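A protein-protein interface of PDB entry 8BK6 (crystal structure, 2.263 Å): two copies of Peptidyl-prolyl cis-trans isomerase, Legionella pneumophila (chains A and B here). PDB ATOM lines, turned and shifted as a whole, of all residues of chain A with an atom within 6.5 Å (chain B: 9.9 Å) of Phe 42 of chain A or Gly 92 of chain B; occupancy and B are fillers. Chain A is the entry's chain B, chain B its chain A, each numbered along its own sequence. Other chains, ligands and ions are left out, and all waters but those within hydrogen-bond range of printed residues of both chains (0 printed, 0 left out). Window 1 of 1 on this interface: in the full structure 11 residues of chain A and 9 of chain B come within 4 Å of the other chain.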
ATOM      1  N   TYR A  32      23.224 -12.866 -34.541  1.00  0.00           N
ATOM      2  CA  TYR A  32      24.198 -13.765 -33.946  1.00  0.00           C
ATOM      3  C   TYR A  32      23.556 -15.091 -33.562  1.00  0.00           C
ATOM      4  O   TYR A  32      22.342 -15.194 -33.376  1.00  0.00           O
ATOM      5  CB  TYR A  32      24.871 -13.145 -32.712  1.00  0.00           C
ATOM      6  CG  TYR A  32      23.996 -13.040 -31.470  1.00  0.00           C
ATOM      7  CD1 TYR A  32      23.828 -14.130 -30.615  1.00  0.00           C
ATOM      8  CD2 TYR A  32      23.390 -11.840 -31.116  1.00  0.00           C
ATOM      9  CE1 TYR A  32      23.040 -14.039 -29.475  1.00  0.00           C
ATOM     10  CE2 TYR A  32      22.606 -11.738 -29.978  1.00  0.00           C
ATOM     11  CZ  TYR A  32      22.438 -12.840 -29.157  1.00  0.00           C
ATOM     12  OH  TYR A  32      21.664 -12.758 -28.017  1.00  0.00           O
ATOM     13  N   THR A  33      24.415 -16.100 -33.440  1.00  0.00           N
ATOM     14  CA  THR A  33      24.090 -17.394 -32.846  1.00  0.00           C
ATOM     15  C   THR A  33      25.265 -17.772 -31.959  1.00  0.00           C
ATOM     16  O   THR A  33      26.412 -17.731 -32.413  1.00  0.00           O
ATOM     17  CB  THR A  33      23.849 -18.471 -33.913  1.00  0.00           C
ATOM     18  OG1 THR A  33      22.925 -17.975 -34.898  1.00  0.00           O
ATOM     19  CG2 THR A  33      23.288 -19.744 -33.279  1.00  0.00           C
ATOM     20  N   GLY A  34      24.984 -18.082 -30.698  1.00  0.00           N
ATOM     21  CA  GLY A  34      25.999 -18.488 -29.733  1.00  0.00           C
ATOM     22  C   GLY A  34      25.847 -19.954 -29.347  1.00  0.00           C
ATOM     23  O   GLY A  34      24.727 -20.431 -29.132  1.00  0.00           O
ATOM     24  N   ARG A  35      26.981 -20.657 -29.267  1.00  0.00           N
ATOM     25  CA  ARG A  35      26.989 -22.090 -28.988  1.00  0.00           C
ATOM     26  C   ARG A  35      28.210 -22.468 -28.151  1.00  0.00           C
ATOM     27  O   ARG A  35      29.197 -21.733 -28.086  1.00  0.00           O
ATOM     28  CB  ARG A  35      26.956 -22.913 -30.290  1.00  0.00           C
ATOM     29  CG  ARG A  35      28.238 -22.867 -31.125  1.00  0.00           C
ATOM     30  CD  ARG A  35      28.090 -23.705 -32.396  1.00  0.00           C
ATOM     31  NE  ARG A  35      29.356 -23.911 -33.090  1.00  0.00           N
ATOM     32  CZ  ARG A  35      29.768 -23.216 -34.148  1.00  0.00           C
ATOM     33  NH1 ARG A  35      29.196 -22.071 -34.494  1.00  0.00           N
ATOM     34  NH2 ARG A  35      30.843 -23.630 -34.819  1.00  0.00           N
ATOM     35  N   LEU A  36      28.127 -23.634 -27.506  1.00  0.00           N
ATOM     36  CA  LEU A  36      29.241 -24.208 -26.767  1.00  0.00           C
ATOM     37  C   LEU A  36      30.030 -25.154 -27.679  1.00  0.00           C
ATOM     38  O   LEU A  36      29.639 -25.425 -28.817  1.00  0.00           O
ATOM     39  CB  LEU A  36      28.741 -24.938 -25.524  1.00  0.00           C
ATOM     40  CG  LEU A  36      27.634 -24.233 -24.754  1.00  0.00           C
ATOM     41  CD1 LEU A  36      26.999 -25.194 -23.754  1.00  0.00           C
ATOM     42  CD2 LEU A  36      28.205 -23.023 -24.061  1.00  0.00           C
ATOM     43  N   GLY A  39      28.255 -27.933 -29.170  1.00  0.00           N
ATOM     44  CA  GLY A  39      27.300 -27.540 -30.185  1.00  0.00           C
ATOM     45  C   GLY A  39      25.955 -27.085 -29.666  1.00  0.00           C
ATOM     46  O   GLY A  39      25.109 -26.696 -30.482  1.00  0.00           O
ATOM     47  N   THR A  40      25.720 -27.132 -28.349  1.00  0.00           N
ATOM     48  CA  THR A  40      24.487 -26.598 -27.768  1.00  0.00           C
ATOM     49  C   THR A  40      24.373 -25.099 -28.028  1.00  0.00           C
ATOM     50  O   THR A  40      25.249 -24.330 -27.622  1.00  0.00           O
ATOM     51  CB  THR A  40      24.438 -26.853 -26.252  1.00  0.00           C
ATOM     52  OG1 THR A  40      24.890 -28.181 -25.932  1.00  0.00           O
ATOM     53  CG2 THR A  40      23.032 -26.625 -25.714  1.00  0.00           C
ATOM     54  N   VAL A  41      23.306 -24.681 -28.713  1.00  0.00           N
ATOM     55  CA  VAL A  41      23.035 -23.257 -28.907  1.00  0.00           C
ATOM     56  C   VAL A  41      22.396 -22.683 -27.649  1.00  0.00           C
ATOM     57  O   VAL A  41      21.392 -23.212 -27.155  1.00  0.00           O
ATOM     58  CB  VAL A  41      22.142 -23.032 -30.134  1.00  0.00           C
ATOM     59  CG1 VAL A  41      21.791 -21.554 -30.280  1.00  0.00           C
ATOM     60  CG2 VAL A  41      22.847 -23.527 -31.372  1.00  0.00           C
ATOM     61  N   PHE A  42      22.983 -21.612 -27.107  1.00  0.00           N
ATOM     62  CA  PHE A  42      22.409 -21.022 -25.901  1.00  0.00           C
ATOM     63  C   PHE A  42      21.541 -19.791 -26.156  1.00  0.00           C
ATOM     64  O   PHE A  42      20.653 -19.505 -25.343  1.00  0.00           O
ATOM     65  CB  PHE A  42      23.486 -20.696 -24.846  1.00  0.00           C
ATOM     66  CG  PHE A  42      24.709 -19.975 -25.354  1.00  0.00           C
ATOM     67  CD1 PHE A  42      24.706 -18.595 -25.528  1.00  0.00           C
ATOM     68  CD2 PHE A  42      25.898 -20.666 -25.572  1.00  0.00           C
ATOM     69  CE1 PHE A  42      25.862 -17.916 -25.954  1.00  0.00           C
ATOM     70  CE2 PHE A  42      27.053 -19.999 -26.006  1.00  0.00           C
ATOM     71  CZ  PHE A  42      27.032 -18.623 -26.204  1.00  0.00           C
ATOM     72  N   ASP A  43      21.813 -19.092 -27.258  1.00  0.00           N
ATOM     73  CA  ASP A  43      21.017 -17.900 -27.639  1.00  0.00           C
ATOM     74  C   ASP A  43      21.231 -17.631 -29.121  1.00  0.00           C
ATOM     75  O   ASP A  43      22.298 -17.979 -29.637  1.00  0.00           O
ATOM     76  CB  ASP A  43      21.377 -16.657 -26.826  1.00  0.00           C
ATOM     77  CG  ASP A  43      20.228 -15.697 -26.567  1.00  0.00           C
ATOM     78  OD1 ASP A  43      19.059 -16.131 -26.619  1.00  0.00           O
ATOM     79  OD2 ASP A  43      20.516 -14.519 -26.297  1.00  0.00           O
ATOM     80  N   SER A  44      20.244 -17.018 -29.750  1.00  0.00           N
ATOM     81  CA  SER A  44      20.314 -16.720 -31.170  1.00  0.00           C
ATOM     82  C   SER A  44      19.415 -15.519 -31.422  1.00  0.00           C
ATOM     83  O   SER A  44      18.438 -15.314 -30.700  1.00  0.00           O
ATOM     84  CB  SER A  44      19.869 -17.926 -32.011  1.00  0.00           C
ATOM     85  OG  SER A  44      20.421 -17.881 -33.310  1.00  0.00           O
ATOM     86  N   LYS A  47      16.040 -17.021 -32.708  1.00  0.00           N
ATOM     87  CA  LYS A  47      15.022 -17.443 -31.748  1.00  0.00           C
ATOM     88  C   LYS A  47      14.069 -16.297 -31.405  1.00  0.00           C
ATOM     89  O   LYS A  47      12.932 -16.549 -30.989  1.00  0.00           O
ATOM     90  CB  LYS A  47      15.690 -18.028 -30.500  1.00  0.00           C
ATOM     91  CG  LYS A  47      16.452 -19.312 -30.821  1.00  0.00           C
ATOM     92  CD  LYS A  47      17.251 -19.890 -29.653  1.00  0.00           C
ATOM     93  CE  LYS A  47      17.079 -21.414 -29.593  1.00  0.00           C
ATOM     94  NZ  LYS A  47      18.333 -22.154 -29.944  1.00  0.00           N
ATOM     95  N   TYR A  86      32.315 -15.192 -19.760  1.00  0.00           N
ATOM     96  CA  TYR A  86      31.759 -15.129 -18.416  1.00  0.00           C
ATOM     97  C   TYR A  86      32.676 -15.760 -17.374  1.00  0.00           C
ATOM     98  O   TYR A  86      32.319 -15.788 -16.194  1.00  0.00           O
ATOM     99  CB  TYR A  86      30.366 -15.775 -18.386  1.00  0.00           C
ATOM    100  CG  TYR A  86      29.382 -14.999 -19.223  1.00  0.00           C
ATOM    101  CD1 TYR A  86      28.731 -13.873 -18.717  1.00  0.00           C
ATOM    102  CD2 TYR A  86      29.142 -15.358 -20.540  1.00  0.00           C
ATOM    103  CE1 TYR A  86      27.844 -13.143 -19.497  1.00  0.00           C
ATOM    104  CE2 TYR A  86      28.264 -14.639 -21.327  1.00  0.00           C
ATOM    105  CZ  TYR A  86      27.614 -13.532 -20.807  1.00  0.00           C
ATOM    106  OH  TYR A  86      26.745 -12.830 -21.616  1.00  0.00           O
ATOM    107  N   VAL A  91      27.011 -19.203 -15.397  1.00  0.00           N
ATOM    108  CA  VAL A  91      25.802 -18.388 -15.462  1.00  0.00           C
ATOM    109  C   VAL A  91      24.698 -19.046 -14.644  1.00  0.00           C
ATOM    110  O   VAL A  91      23.534 -18.621 -14.700  1.00  0.00           O
ATOM    111  CB  VAL A  91      25.344 -18.148 -16.914  1.00  0.00           C
ATOM    112  CG1 VAL A  91      26.500 -17.607 -17.748  1.00  0.00           C
ATOM    113  CG2 VAL A  91      24.743 -19.423 -17.509  1.00  0.00           C
ATOM    114  N   GLY A  92      25.051 -20.085 -13.876  1.00  0.00           N
ATOM    115  CA  GLY A  92      24.054 -20.789 -13.095  1.00  0.00           C
ATOM    116  C   GLY A  92      23.230 -21.745 -13.921  1.00  0.00           C
ATOM    117  O   GLY A  92      22.208 -22.253 -13.436  1.00  0.00           O
ATOM    118  N   GLY A  93      23.597 -21.884 -15.201  1.00  0.00           N
ATOM    119  CA  GLY A  93      22.847 -22.756 -16.122  1.00  0.00           C
ATOM    120  C   GLY A  93      23.757 -23.355 -17.180  1.00  0.00           C
ATOM    121  O   GLY A  93      24.970 -23.441 -16.931  1.00  0.00           O
ATOM    122  N   PRO A  94      23.230 -23.774 -18.348  1.00  0.00           N
ATOM    123  CA  PRO A  94      24.029 -24.424 -19.396  1.00  0.00           C
ATOM    124  C   PRO A  94      25.473 -23.940 -19.573  1.00  0.00           C
ATOM    125  O   PRO A  94      26.325 -24.786 -19.722  1.00  0.00           O
ATOM    126  CB  PRO A  94      23.233 -24.049 -20.654  1.00  0.00           C
ATOM    127  CG  PRO A  94      21.796 -24.096 -20.189  1.00  0.00           C
ATOM    128  CD  PRO A  94      21.824 -23.677 -18.733  1.00  0.00           C
ATOM    129  N   ILE A  95      25.718 -22.629 -19.550  1.00  0.00           N
ATOM    130  CA  ILE A  95      27.069 -22.147 -19.846  1.00  0.00           C
ATOM    131  C   ILE A  95      28.076 -22.852 -18.947  1.00  0.00           C
ATOM    132  O   ILE A  95      28.998 -23.533 -19.414  1.00  0.00           O
ATOM    133  CB  ILE A  95      27.148 -20.615 -19.706  1.00  0.00           C
ATOM    134  CG1 ILE A  95      26.383 -19.940 -20.849  1.00  0.00           C
ATOM    135  CG2 ILE A  95      28.592 -20.123 -19.665  1.00  0.00           C
ATOM    136  CD1 ILE A  95      27.070 -20.009 -22.188  1.00  0.00           C
ATOM    137  N   THR A 100      34.291 -22.093 -22.927  1.00  0.00           N
ATOM    138  CA  THR A 100      34.583 -21.416 -24.185  1.00  0.00           C
ATOM    139  C   THR A 100      33.304 -21.281 -25.014  1.00  0.00           C
ATOM    140  O   THR A 100      32.495 -22.212 -25.097  1.00  0.00           O
ATOM    141  CB  THR A 100      35.660 -22.183 -24.960  1.00  0.00           C
ATOM    142  OG1 THR A 100      36.925 -22.000 -24.319  1.00  0.00           O
ATOM    143  CG2 THR A 100      35.776 -21.682 -26.407  1.00  0.00           C
ATOM    144  N   LEU A 101      33.124 -20.116 -25.635  1.00  0.00           N
ATOM    145  CA  LEU A 101      31.919 -19.811 -26.398  1.00  0.00           C
ATOM    146  C   LEU A 101      32.295 -19.510 -27.841  1.00  0.00           C
ATOM    147  O   LEU A 101      33.326 -18.884 -28.105  1.00  0.00           O
ATOM    148  CB  LEU A 101      31.149 -18.622 -25.804  1.00  0.00           C
ATOM    149  CG  LEU A 101      31.021 -18.552 -24.284  1.00  0.00           C
ATOM    150  CD1 LEU A 101      30.190 -17.331 -23.844  1.00  0.00           C
ATOM    151  CD2 LEU A 101      30.406 -19.856 -23.773  1.00  0.00           C
ATOM    152  N   ILE A 102      31.482 -20.017 -28.765  1.00  0.00           N
ATOM    153  CA  ILE A 102      31.617 -19.759 -30.194  1.00  0.00           C
ATOM    154  C   ILE A 102      30.408 -18.953 -30.648  1.00  0.00           C
ATOM    155  O   ILE A 102      29.262 -19.363 -30.424  1.00  0.00           O
ATOM    156  CB  ILE A 102      31.743 -21.064 -30.998  1.00  0.00           C
ATOM    157  CG1 ILE A 102      32.993 -21.843 -30.569  1.00  0.00           C
ATOM    158  CG2 ILE A 102      31.785 -20.773 -32.486  1.00  0.00           C
ATOM    159  CD1 ILE A 102      32.717 -22.957 -29.591  1.00  0.00           C
ATOM    160  N   PHE A 103      30.665 -17.821 -31.309  1.00  0.00           N
ATOM    161  CA  PHE A 103      29.623 -16.927 -31.801  1.00  0.00           C
ATOM    162  C   PHE A 103      29.768 -16.752 -33.306  1.00  0.00           C
ATOM    163  O   PHE A 103      30.871 -16.491 -33.797  1.00  0.00           O
ATOM    164  CB  PHE A 103      29.695 -15.551 -31.120  1.00  0.00           C
ATOM    165  CG  PHE A 103      29.242 -15.542 -29.680  1.00  0.00           C
ATOM    166  CD1 PHE A 103      27.898 -15.360 -29.358  1.00  0.00           C
ATOM    167  CD2 PHE A 103      30.165 -15.649 -28.648  1.00  0.00           C
ATOM    168  CE1 PHE A 103      27.479 -15.322 -28.031  1.00  0.00           C
ATOM    169  CE2 PHE A 103      29.755 -15.606 -27.317  1.00  0.00           C
ATOM    170  CZ  PHE A 103      28.410 -15.442 -27.012  1.00  0.00           C
ATOM    171  N   PHE B  42      19.444 -15.291 -11.148  1.00  0.00           N
ATOM    172  CA  PHE B  42      19.926 -15.763 -12.471  1.00  0.00           C
ATOM    173  C   PHE B  42      20.937 -14.776 -13.075  1.00  0.00           C
ATOM    174  O   PHE B  42      21.899 -15.255 -13.692  1.00  0.00           O
ATOM    175  CB  PHE B  42      18.741 -16.121 -13.374  1.00  0.00           C
ATOM    176  CG  PHE B  42      17.613 -15.134 -13.501  1.00  0.00           C
ATOM    177  CD1 PHE B  42      17.725 -14.026 -14.321  1.00  0.00           C
ATOM    178  CD2 PHE B  42      16.407 -15.361 -12.863  1.00  0.00           C
ATOM    179  CE1 PHE B  42      16.669 -13.143 -14.459  1.00  0.00           C
ATOM    180  CE2 PHE B  42      15.349 -14.483 -13.013  1.00  0.00           C
ATOM    181  CZ  PHE B  42      15.483 -13.372 -13.806  1.00  0.00           C
ATOM    182  N   ASP B  43      20.733 -13.469 -12.922  1.00  0.00           N
ATOM    183  CA  ASP B  43      21.745 -12.482 -13.385  1.00  0.00           C
ATOM    184  C   ASP B  43      21.646 -11.254 -12.481  1.00  0.00           C
ATOM    185  O   ASP B  43      20.577 -11.035 -11.894  1.00  0.00           O
ATOM    186  CB  ASP B  43      21.624 -12.107 -14.866  1.00  0.00           C
ATOM    187  CG  ASP B  43      22.814 -11.346 -15.439  1.00  0.00           C
ATOM    188  OD1 ASP B  43      23.956 -11.860 -15.384  1.00  0.00           O
ATOM    189  OD2 ASP B  43      22.589 -10.244 -15.959  1.00  0.00           O
ATOM    190  N   TYR B  86      10.244 -15.063 -21.133  1.00  0.00           N
ATOM    191  CA  TYR B  86      10.840 -15.988 -22.135  1.00  0.00           C
ATOM    192  C   TYR B  86       9.809 -17.014 -22.613  1.00  0.00           C
ATOM    193  O   TYR B  86      10.141 -17.802 -23.506  1.00  0.00           O
ATOM    194  CB  TYR B  86      12.143 -16.496 -21.516  1.00  0.00           C
ATOM    195  CG  TYR B  86      13.217 -15.423 -21.411  1.00  0.00           C
ATOM    196  CD1 TYR B  86      13.763 -14.847 -22.548  1.00  0.00           C
ATOM    197  CD2 TYR B  86      13.678 -14.983 -20.177  1.00  0.00           C
ATOM    198  CE1 TYR B  86      14.744 -13.875 -22.465  1.00  0.00           C
ATOM    199  CE2 TYR B  86      14.656 -14.010 -20.080  1.00  0.00           C
ATOM    200  CZ  TYR B  86      15.191 -13.454 -21.227  1.00  0.00           C
ATOM    201  OH  TYR B  86      16.152 -12.493 -21.144  1.00  0.00           O
ATOM    202  N   ARG B  89       9.756 -21.130 -23.966  1.00  0.00           N
ATOM    203  CA  ARG B  89      11.147 -21.494 -24.308  1.00  0.00           C
ATOM    204  C   ARG B  89      12.006 -21.522 -23.045  1.00  0.00           C
ATOM    205  O   ARG B  89      11.792 -20.678 -22.169  1.00  0.00           O
ATOM    206  CB  ARG B  89      11.696 -20.492 -25.323  1.00  0.00           C
ATOM    207  CG  ARG B  89      10.623 -19.833 -26.176  1.00  0.00           C
ATOM    208  CD  ARG B  89      11.227 -19.067 -27.335  1.00  0.00           C
ATOM    209  NE  ARG B  89      11.568 -19.947 -28.443  1.00  0.00           N
ATOM    210  CZ  ARG B  89      10.708 -20.760 -29.042  1.00  0.00           C
ATOM    211  NH1 ARG B  89       9.626 -20.269 -29.618  1.00  0.00           N
ATOM    212  NH2 ARG B  89      10.929 -22.063 -29.060  1.00  0.00           N
ATOM    213  N   SER B  90      12.900 -22.502 -22.945  1.00  0.00           N
ATOM    214  CA  SER B  90      13.873 -22.512 -21.828  1.00  0.00           C
ATOM    215  C   SER B  90      15.090 -21.725 -22.315  1.00  0.00           C
ATOM    216  O   SER B  90      15.573 -22.034 -23.412  1.00  0.00           O
ATOM    217  CB  SER B  90      14.224 -23.908 -21.414  1.00  0.00           C
ATOM    218  OG  SER B  90      13.053 -24.674 -21.179  1.00  0.00           O
ATOM    219  N   VAL B  91      15.546 -20.736 -21.549  1.00  0.00           N
ATOM    220  CA  VAL B  91      16.644 -19.843 -22.030  1.00  0.00           C
ATOM    221  C   VAL B  91      17.946 -20.125 -21.272  1.00  0.00           C
ATOM    222  O   VAL B  91      17.957 -19.944 -20.048  1.00  0.00           O
ATOM    223  CB  VAL B  91      16.217 -18.366 -21.950  1.00  0.00           C
ATOM    224  CG1 VAL B  91      15.424 -17.966 -23.183  1.00  0.00           C
ATOM    225  CG2 VAL B  91      15.412 -18.085 -20.696  1.00  0.00           C
ATOM    226  N   GLY B  92      18.994 -20.545 -21.985  1.00  0.00           N
ATOM    227  CA  GLY B  92      20.309 -20.872 -21.390  1.00  0.00           C
ATOM    228  C   GLY B  92      20.458 -20.523 -19.922  1.00  0.00           C
ATOM    229  O   GLY B  92      21.151 -19.539 -19.621  1.00  0.00           O
ATOM    230  N   GLY B  93      19.874 -21.329 -19.037  1.00  0.00           N
ATOM    231  CA  GLY B  93      20.010 -21.103 -17.586  1.00  0.00           C
ATOM    232  C   GLY B  93      19.024 -21.940 -16.799  1.00  0.00           C
ATOM    233  O   GLY B  93      18.327 -22.769 -17.411  1.00  0.00           O
ATOM    234  N   PRO B  94      18.900 -21.738 -15.470  1.00  0.00           N
ATOM    235  CA  PRO B  94      17.912 -22.456 -14.678  1.00  0.00           C
ATOM    236  C   PRO B  94      16.528 -21.975 -15.118  1.00  0.00           C
ATOM    237  O   PRO B  94      15.549 -22.573 -14.712  1.00  0.00           O
ATOM    238  CB  PRO B  94      18.213 -22.023 -13.242  1.00  0.00           C
ATOM    239  CG  PRO B  94      18.872 -20.670 -13.397  1.00  0.00           C
ATOM    240  CD  PRO B  94      19.661 -20.766 -14.685  1.00  0.00           C
ATOM    241  N   ILE B  95      16.488 -20.907 -15.917  1.00  0.00           N
ATOM    242  CA  ILE B  95      15.191 -20.426 -16.458  1.00  0.00           C
ATOM    243  C   ILE B  95      14.704 -21.511 -17.413  1.00  0.00           C
ATOM    244  O   ILE B  95      15.374 -21.752 -18.428  1.00  0.00           O
ATOM    245  CB  ILE B  95      15.321 -19.051 -17.134  1.00  0.00           C
ATOM    246  CG1 ILE B  95      16.135 -18.081 -16.277  1.00  0.00           C
ATOM    247  CG2 ILE B  95      13.951 -18.493 -17.472  1.00  0.00           C
ATOM    248  CD1 ILE B  95      15.759 -16.634 -16.476  1.00  0.00           C
ATOM    249  N   GLY B  96      13.612 -22.171 -17.044  1.00  0.00           N
ATOM    250  CA  GLY B  96      13.052 -23.227 -17.896  1.00  0.00           C
ATOM    251  C   GLY B  96      11.806 -22.756 -18.612  1.00  0.00           C
ATOM    252  O   GLY B  96      11.669 -21.550 -18.842  1.00  0.00           O
ATOM    253  N   PRO B  97      10.892 -23.676 -18.963  1.00  0.00           N
ATOM    254  CA  PRO B  97       9.696 -23.314 -19.699  1.00  0.00           C
ATOM    255  C   PRO B  97       8.643 -22.614 -18.828  1.00  0.00           C
ATOM    256  O   PRO B  97       8.454 -23.006 -17.703  1.00  0.00           O
ATOM    257  CB  PRO B  97       9.204 -24.674 -20.214  1.00  0.00           C
ATOM    258  CG  PRO B  97       9.667 -25.662 -19.175  1.00  0.00           C
ATOM    259  CD  PRO B  97      10.976 -25.103 -18.662  1.00  0.00           C
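Of the 12 printed residues of chain B, 4 touch a printed residue of chain A.
Hydrophobic or aromatic side chains of chain B that line the printed part of chain A: Pro 94.
Printed residues of chain A that touch a printed residue of chain B: Phe 42, Val 91, Gly 92, Gly 93 and Pro 94.
Hydrophobic or aromatic side chains of chain A that line the printed part of chain B: Pro 94.
Among the printed residues, 6 pairs touch across the chains.
Among the printed residues, no Asp or Glu carboxylate lies within 4 Å of a Lys or Arg side-chain nitrogen of the other chain.
Phe 42 of chain A touches Gly 92 of chain B, but with the chains exchanged Gly 92 of chain A does not touch Phe 42 of chain B (5.8 Å).
Val 91 of chain A touches Phe 42 of chain B, but with the chains exchanged Phe 42 of chain A does not touch Val 91 of chain B (4.9 Å).
Gly 92 of chain A touches Pro 94 of chain B, and with the chains exchanged Pro 94 of chain A touches Gly 92 of chain B.
Gly 93 of chain A touches its own counterpart, Gly 93 of chain B.
Positions printed for both chains: 42, 43, 86, 91, 92, 93, 94 and 95.
Of the 6 pairs that touch across the chains among the printed residues, 3 have their exchanged pair printed and touching as well.
The backbone carbonyl oxygen (O) of Gly 34 of chain A lies within hydrogen-bond range of the backbone NH (N) of Phe 42 of chain A (2.9 Å).
Among the printed residues, merely in contact across the chains: Phe 42 of chain A with Gly 92 of chain B, Val 91 of chain A with Phe 42 of chain B, Gly 92 of chain A with Pro 94 of chain B, Gly 93 of chain A with Gly 93 of chain B, Pro 94 of chain A with Gly 92 of chain B and Pro 94 of chain A with Gly 93 of chain B.
Phe 42 of chain A touches just one residue of chain B: Gly 92 (3.9 Å).
Gly 92 of chain B touches just these residues of chain A: Phe 42 and Pro 94.
Val 41 of chain A touches none of the printed residues of chain B.
Of the printed residues of chain B, Val 91 of chain A touches Phe 42.
Printed residues of chain B within 4 Å of Gly 92 of chain A: Pro 94.
Printed residues of chain B within 4 Å of Gly 93 of chain A: Gly 93.
Ser 44 of chain A touches none of the printed residues of chain B.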
